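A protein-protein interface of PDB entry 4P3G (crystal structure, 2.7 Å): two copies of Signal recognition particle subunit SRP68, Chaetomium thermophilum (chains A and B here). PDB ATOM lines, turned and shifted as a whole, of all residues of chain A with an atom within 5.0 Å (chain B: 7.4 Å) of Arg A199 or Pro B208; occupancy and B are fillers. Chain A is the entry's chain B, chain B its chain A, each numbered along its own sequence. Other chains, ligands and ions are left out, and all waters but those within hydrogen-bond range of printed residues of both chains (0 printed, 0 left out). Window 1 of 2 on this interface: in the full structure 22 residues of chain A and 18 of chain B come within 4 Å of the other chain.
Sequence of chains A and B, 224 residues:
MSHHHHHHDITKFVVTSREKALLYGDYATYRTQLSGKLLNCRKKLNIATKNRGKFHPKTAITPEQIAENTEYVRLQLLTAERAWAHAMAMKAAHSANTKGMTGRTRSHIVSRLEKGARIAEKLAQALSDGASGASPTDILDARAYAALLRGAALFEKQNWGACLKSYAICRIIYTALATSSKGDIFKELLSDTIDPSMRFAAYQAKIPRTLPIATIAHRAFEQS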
ATOM      1  N   ASP A 195       4.988   1.711 -37.514  1.00  0.00           N
ATOM      2  CA  ASP A 195       4.784   2.343 -36.214  1.00  0.00           C
ATOM      3  C   ASP A 195       5.159   1.464 -35.022  1.00  0.00           C
ATOM      4  O   ASP A 195       5.945   1.891 -34.177  1.00  0.00           O
ATOM      5  CB  ASP A 195       3.373   2.914 -36.084  1.00  0.00           C
ATOM      6  CG  ASP A 195       3.201   4.234 -36.848  1.00  0.00           C
ATOM      7  OD1 ASP A 195       4.154   4.661 -37.549  1.00  0.00           O
ATOM      8  OD2 ASP A 195       2.108   4.844 -36.750  1.00  0.00           O
ATOM      9  N   PRO A 196       4.656   0.219 -34.961  1.00  0.00           N
ATOM     10  CA  PRO A 196       5.048  -0.537 -33.768  1.00  0.00           C
ATOM     11  C   PRO A 196       6.568  -0.757 -33.695  1.00  0.00           C
ATOM     12  O   PRO A 196       7.095  -0.777 -32.581  1.00  0.00           O
ATOM     13  CB  PRO A 196       4.326  -1.863 -33.941  1.00  0.00           C
ATOM     14  CG  PRO A 196       3.242  -1.602 -34.941  1.00  0.00           C
ATOM     15  CD  PRO A 196       3.769  -0.563 -35.844  1.00  0.00           C
ATOM     16  N   SER A 197       7.247  -0.896 -34.841  1.00  0.00           N
ATOM     17  CA  SER A 197       8.702  -1.086 -34.875  1.00  0.00           C
ATOM     18  C   SER A 197       9.492   0.125 -34.423  1.00  0.00           C
ATOM     19  O   SER A 197      10.556   0.000 -33.832  1.00  0.00           O
ATOM     20  CB  SER A 197       9.168  -1.457 -36.269  1.00  0.00           C
ATOM     21  OG  SER A 197       8.581  -2.680 -36.682  1.00  0.00           O
ATOM     22  N   MET A 198       8.981   1.310 -34.705  1.00  0.00           N
ATOM     23  CA  MET A 198       9.677   2.511 -34.297  1.00  0.00           C
ATOM     24  C   MET A 198       9.462   2.779 -32.816  1.00  0.00           C
ATOM     25  O   MET A 198      10.331   3.332 -32.161  1.00  0.00           O
ATOM     26  CB  MET A 198       9.195   3.700 -35.101  1.00  0.00           C
ATOM     27  CG  MET A 198       9.388   3.558 -36.596  1.00  0.00           C
ATOM     28  SD  MET A 198       9.026   5.292 -37.466  1.00  0.00           S
ATOM     29  CE  MET A 198      10.693   6.156 -37.032  1.00  0.00           C
ATOM     30  N   ARG A 199       8.301   2.411 -32.288  1.00  0.00           N
ATOM     31  CA  ARG A 199       8.074   2.604 -30.870  1.00  0.00           C
ATOM     32  C   ARG A 199       9.044   1.752 -30.067  1.00  0.00           C
ATOM     33  O   ARG A 199       9.591   2.199 -29.071  1.00  0.00           O
ATOM     34  CB  ARG A 199       6.652   2.234 -30.488  1.00  0.00           C
ATOM     35  CG  ARG A 199       5.659   3.073 -31.133  1.00  0.00           C
ATOM     36  CD  ARG A 199       4.472   3.293 -30.262  1.00  0.00           C
ATOM     37  NE  ARG A 199       3.644   4.283 -30.931  1.00  0.00           N
ATOM     38  CZ  ARG A 199       2.541   4.813 -30.432  1.00  0.00           C
ATOM     39  NH1 ARG A 199       2.124   4.461 -29.227  1.00  0.00           N
ATOM     40  NH2 ARG A 199       1.872   5.712 -31.141  1.00  0.00           N
ATOM     41  N   PHE A 200       9.263   0.525 -30.520  1.00  0.00           N
ATOM     42  CA  PHE A 200      10.164  -0.383 -29.839  1.00  0.00           C
ATOM     43  C   PHE A 200      11.595   0.120 -29.926  1.00  0.00           C
ATOM     44  O   PHE A 200      12.283   0.228 -28.917  1.00  0.00           O
ATOM     45  CB  PHE A 200      10.061  -1.774 -30.442  1.00  0.00           C
ATOM     46  CG  PHE A 200      10.823  -2.817 -29.700  1.00  0.00           C
ATOM     47  CD1 PHE A 200      10.276  -3.415 -28.586  1.00  0.00           C
ATOM     48  CD2 PHE A 200      12.064  -3.231 -30.133  1.00  0.00           C
ATOM     49  CE1 PHE A 200      10.965  -4.416 -27.896  1.00  0.00           C
ATOM     50  CE2 PHE A 200      12.759  -4.226 -29.449  1.00  0.00           C
ATOM     51  CZ  PHE A 200      12.205  -4.812 -28.327  1.00  0.00           C
ATOM     52  N   ALA A 201      12.042   0.435 -31.135  1.00  0.00           N
ATOM     53  CA  ALA A 201      13.412   0.892 -31.319  1.00  0.00           C
ATOM     54  C   ALA A 201      13.671   2.162 -30.511  1.00  0.00           C
ATOM     55  O   ALA A 201      14.758   2.378 -29.997  1.00  0.00           O
ATOM     56  CB  ALA A 201      13.699   1.124 -32.785  1.00  0.00           C
ATOM     57  N   ALA A 202      12.667   3.016 -30.413  1.00  0.00           N
ATOM     58  CA  ALA A 202      12.811   4.242 -29.659  1.00  0.00           C
ATOM     59  C   ALA A 202      12.860   3.955 -28.147  1.00  0.00           C
ATOM     60  O   ALA A 202      13.623   4.572 -27.404  1.00  0.00           O
ATOM     61  CB  ALA A 202      11.681   5.219 -30.017  1.00  0.00           C
ATOM     62  N   TYR A 203      12.039   3.021 -27.692  1.00  0.00           N
ATOM     63  CA  TYR A 203      12.109   2.606 -26.309  1.00  0.00           C
ATOM     64  C   TYR A 203      13.512   2.087 -25.995  1.00  0.00           C
ATOM     65  O   TYR A 203      14.126   2.506 -25.027  1.00  0.00           O
ATOM     66  CB  TYR A 203      11.090   1.522 -26.039  1.00  0.00           C
ATOM     67  CG  TYR A 203      11.240   0.911 -24.669  1.00  0.00           C
ATOM     68  CD1 TYR A 203      10.923   1.626 -23.529  1.00  0.00           C
ATOM     69  CD2 TYR A 203      11.724  -0.394 -24.520  1.00  0.00           C
ATOM     70  CE1 TYR A 203      11.060   1.078 -22.287  1.00  0.00           C
ATOM     71  CE2 TYR A 203      11.864  -0.958 -23.279  1.00  0.00           C
ATOM     72  CZ  TYR A 203      11.534  -0.222 -22.158  1.00  0.00           C
ATOM     73  OH  TYR A 203      11.679  -0.786 -20.909  1.00  0.00           O
ATOM     74  N   PRO A 212       8.909  12.279 -21.332  1.00  0.00           N
ATOM     75  CA  PRO A 212       7.710  13.084 -21.633  1.00  0.00           C
ATOM     76  C   PRO A 212       6.691  13.129 -20.501  1.00  0.00           C
ATOM     77  O   PRO A 212       5.543  12.753 -20.723  1.00  0.00           O
ATOM     78  CB  PRO A 212       7.093  12.348 -22.831  1.00  0.00           C
ATOM     79  CG  PRO A 212       7.564  10.941 -22.716  1.00  0.00           C
ATOM     80  CD  PRO A 212       8.975  11.062 -22.165  1.00  0.00           C
ATOM     81  N   THR A 215       3.081  14.789 -20.972  1.00  0.00           N
ATOM     82  CA  THR A 215       2.300  13.992 -21.901  1.00  0.00           C
ATOM     83  C   THR A 215       1.770  12.732 -21.191  1.00  0.00           C
ATOM     84  O   THR A 215       0.619  12.318 -21.372  1.00  0.00           O
ATOM     85  CB  THR A 215       3.171  13.554 -23.067  1.00  0.00           C
ATOM     86  OG1 THR A 215       3.885  14.693 -23.558  1.00  0.00           O
ATOM     87  CG2 THR A 215       2.335  12.965 -24.140  1.00  0.00           C
ATOM     88  N   ALA B 202       4.853   3.287 -20.177  1.00  0.00           N
ATOM     89  CA  ALA B 202       4.366   4.207 -21.199  1.00  0.00           C
ATOM     90  C   ALA B 202       4.413   3.482 -22.544  1.00  0.00           C
ATOM     91  O   ALA B 202       3.474   3.542 -23.332  1.00  0.00           O
ATOM     92  CB  ALA B 202       5.191   5.468 -21.225  1.00  0.00           C
ATOM     93  N   TYR B 203       5.485   2.734 -22.765  1.00  0.00           N
ATOM     94  CA  TYR B 203       5.575   1.907 -23.947  1.00  0.00           C
ATOM     95  C   TYR B 203       4.414   0.919 -24.016  1.00  0.00           C
ATOM     96  O   TYR B 203       3.768   0.796 -25.050  1.00  0.00           O
ATOM     97  CB  TYR B 203       6.875   1.128 -23.948  1.00  0.00           C
ATOM     98  CG  TYR B 203       6.921   0.156 -25.084  1.00  0.00           C
ATOM     99  CD1 TYR B 203       7.049   0.607 -26.404  1.00  0.00           C
ATOM    100  CD2 TYR B 203       6.776  -1.211 -24.857  1.00  0.00           C
ATOM    101  CE1 TYR B 203       7.059  -0.273 -27.455  1.00  0.00           C
ATOM    102  CE2 TYR B 203       6.782  -2.097 -25.904  1.00  0.00           C
ATOM    103  CZ  TYR B 203       6.924  -1.630 -27.209  1.00  0.00           C
ATOM    104  OH  TYR B 203       6.936  -2.526 -28.262  1.00  0.00           O
ATOM    105  N   ALA B 205       1.544   1.096 -22.641  1.00  0.00           N
ATOM    106  CA  ALA B 205       0.285   1.788 -22.766  1.00  0.00           C
ATOM    107  C   ALA B 205       0.147   2.489 -24.120  1.00  0.00           C
ATOM    108  O   ALA B 205      -0.909   3.062 -24.417  1.00  0.00           O
ATOM    109  CB  ALA B 205       0.118   2.773 -21.609  1.00  0.00           C
ATOM    110  N   LYS B 206       1.208   2.453 -24.929  1.00  0.00           N
ATOM    111  CA  LYS B 206       1.231   3.211 -26.181  1.00  0.00           C
ATOM    112  C   LYS B 206       1.057   4.725 -25.939  1.00  0.00           C
ATOM    113  O   LYS B 206       0.399   5.416 -26.718  1.00  0.00           O
ATOM    114  CB  LYS B 206       0.219   2.670 -27.213  1.00  0.00           C
ATOM    115  CG  LYS B 206       0.724   1.488 -28.069  1.00  0.00           C
ATOM    116  CD  LYS B 206       1.036   0.229 -27.214  1.00  0.00           C
ATOM    117  CE  LYS B 206       1.881  -0.831 -27.962  1.00  0.00           C
ATOM    118  NZ  LYS B 206       2.385  -1.886 -27.024  1.00  0.00           N
ATOM    119  N   ILE B 207       1.568   5.204 -24.806  1.00  0.00           N
ATOM    120  CA  ILE B 207       1.599   6.632 -24.488  1.00  0.00           C
ATOM    121  C   ILE B 207       2.981   7.225 -24.755  1.00  0.00           C
ATOM    122  O   ILE B 207       3.966   6.754 -24.197  1.00  0.00           O
ATOM    123  CB  ILE B 207       1.266   6.878 -23.001  1.00  0.00           C
ATOM    124  CG1 ILE B 207      -0.119   6.320 -22.653  1.00  0.00           C
ATOM    125  CG2 ILE B 207       1.359   8.355 -22.683  1.00  0.00           C
ATOM    126  CD1 ILE B 207      -0.455   6.342 -21.169  1.00  0.00           C
ATOM    127  N   PRO B 208       3.069   8.278 -25.587  1.00  0.00           N
ATOM    128  CA  PRO B 208       2.008   9.040 -26.277  1.00  0.00           C
ATOM    129  C   PRO B 208       1.419   8.347 -27.508  1.00  0.00           C
ATOM    130  O   PRO B 208       2.116   7.561 -28.140  1.00  0.00           O
ATOM    131  CB  PRO B 208       2.729  10.326 -26.714  1.00  0.00           C
ATOM    132  CG  PRO B 208       4.151  10.000 -26.763  1.00  0.00           C
ATOM    133  CD  PRO B 208       4.407   8.857 -25.812  1.00  0.00           C
ATOM    134  N   ARG B 209       0.151   8.637 -27.819  1.00  0.00           N
ATOM    135  CA  ARG B 209      -0.545   8.029 -28.949  1.00  0.00           C
ATOM    136  C   ARG B 209       0.156   8.421 -30.234  1.00  0.00           C
ATOM    137  O   ARG B 209       0.440   7.582 -31.078  1.00  0.00           O
ATOM    138  CB  ARG B 209      -2.003   8.481 -29.015  1.00  0.00           C
ATOM    139  CG  ARG B 209      -2.829   8.201 -27.780  1.00  0.00           C
ATOM    140  CD  ARG B 209      -2.806   6.732 -27.398  1.00  0.00           C
ATOM    141  NE  ARG B 209      -3.531   6.495 -26.150  1.00  0.00           N
ATOM    142  CZ  ARG B 209      -3.369   5.413 -25.398  1.00  0.00           C
ATOM    143  NH1 ARG B 209      -2.506   4.475 -25.774  1.00  0.00           N
ATOM    144  NH2 ARG B 209      -4.060   5.275 -24.273  1.00  0.00           N
ATOM    145  N   THR B 210       0.462   9.702 -30.364  1.00  0.00           N
ATOM    146  CA  THR B 210       1.140  10.205 -31.542  1.00  0.00           C
ATOM    147  C   THR B 210       2.643   9.958 -31.483  1.00  0.00           C
ATOM    148  O   THR B 210       3.322  10.414 -30.567  1.00  0.00           O
ATOM    149  CB  THR B 210       0.853  11.719 -31.703  1.00  0.00           C
ATOM    150  OG1 THR B 210      -0.484  11.884 -32.188  1.00  0.00           O
ATOM    151  CG2 THR B 210       1.822  12.375 -32.673  1.00  0.00           C
ATOM    152  N   LEU B 211       3.171   9.264 -32.485  1.00  0.00           N
ATOM    153  CA  LEU B 211       4.605   8.997 -32.523  1.00  0.00           C
ATOM    154  C   LEU B 211       5.417  10.303 -32.698  1.00  0.00           C
ATOM    155  O   LEU B 211       5.224  11.043 -33.650  1.00  0.00           O
ATOM    156  CB  LEU B 211       4.887   8.101 -33.712  1.00  0.00           C
ATOM    157  CG  LEU B 211       6.188   7.321 -33.820  1.00  0.00           C
ATOM    158  CD1 LEU B 211       6.096   6.160 -32.887  1.00  0.00           C
ATOM    159  CD2 LEU B 211       6.415   6.872 -35.269  1.00  0.00           C
ATOM    160  N   PRO B 212       6.343  10.589 -31.777  1.00  0.00           N
ATOM    161  CA  PRO B 212       7.069  11.853 -31.925  1.00  0.00           C
ATOM    162  C   PRO B 212       8.085  11.687 -33.021  1.00  0.00           C
ATOM    163  O   PRO B 212       9.218  11.341 -32.715  1.00  0.00           O
ATOM    164  CB  PRO B 212       7.777  12.009 -30.574  1.00  0.00           C
ATOM    165  CG  PRO B 212       7.945  10.594 -30.091  1.00  0.00           C
ATOM    166  CD  PRO B 212       6.718   9.862 -30.554  1.00  0.00           C
ATOM    167  N   ILE B 216      12.376  11.988 -33.006  1.00  0.00           N
ATOM    168  CA  ILE B 216      13.102  10.832 -33.482  1.00  0.00           C
ATOM    169  C   ILE B 216      13.959  11.209 -34.683  1.00  0.00           C
ATOM    170  O   ILE B 216      15.140  10.887 -34.723  1.00  0.00           O
ATOM    171  CB  ILE B 216      12.140   9.714 -33.855  1.00  0.00           C
ATOM    172  CG1 ILE B 216      11.548   9.110 -32.580  1.00  0.00           C
ATOM    173  CG2 ILE B 216      12.850   8.662 -34.675  1.00  0.00           C
ATOM    174  CD1 ILE B 216      10.217   8.416 -32.786  1.00  0.00           C
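Positions printed for both chains: 202, 203 and 212. Of the 9 pairs that touch across the chains among the printed residues, none has its exchanged pair printed and touching as well.
O of Ala B205 is in hydrogen-bond range of NH1 of Arg B209. O of Lys B206 is in hydrogen-bond range of NH1 of Arg B209 (3.2 Å).
The backbone carbonyl oxygen (O) of Lys B206 lies within hydrogen-bond range of the guanidinium group (NH1) of Arg A199 (3.2 Å). NH1 of Arg A199 sits at hydrogen-bond distance from O of Pro B208, 3.3 Å away. The backbone carbonyl oxygen (O) of Arg B209 lies close to the guanidinium group (NH2) of Arg A199.
Asp A195 touches Leu B211. Leu B211 touches Met A198. C of Arg A199 touches CE1 of Tyr B203, at 3.9 Å. Arg A199 touches Leu B211 (CG to CD1, 3.6 Å). Tyr B203 touches Phe A200. Thr A215 touches Pro B208.
Printed residues of chain B within 4 Å of Asp A195: Leu B211 (3.9 Å). Pro A196 touches none of the printed residues of chain B. Printed residues of chain B within 4 Å of Met A198: Leu B211 (3.8 Å). Arg A199 touches five residues of chain B. Printed residues of chain B within 4 Å of Phe A200: Tyr B203 (3.5 Å). Printed residues of chain B within 4 Å of Thr A215: Pro B208 (3.7 Å). Ala B205 touches none of the printed residues of chain A. Pro B208 touches just these residues of chain A: Arg A199 and Thr A215. Of the printed residues of chain A, Leu B211 touches Asp A195 (3.9 Å), Met A198 (3.8 Å) and Arg A199 (3.6 Å). The nearest printed residue of chain B that does not touch Met A198 is Ile B216 (4.1 Å).
Printed residues of chain A that touch a printed residue of chain B: Asp A195, Met A198, Arg A199, Phe A200 and Thr A215. Hydrophobic or aromatic side chains of chain A that line the printed part of chain B: Met A198 and Phe A200. Of the 11 printed residues of chain B, 5 touch a printed residue of chain A. Printed residues of chain B that touch a printed residue of chain A: Tyr B203, Lys B206, Pro B208, Arg B209 and Leu B211. Hydrophobic or aromatic side chains of chain B within 4 Å of the printed part of chain A: Tyr B203, Pro B208 and Leu B211. Among the printed residues, no Asp or Glu carboxylate lies within 4 Å of a Lys or Arg side-chain nitrogen of the other chain.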
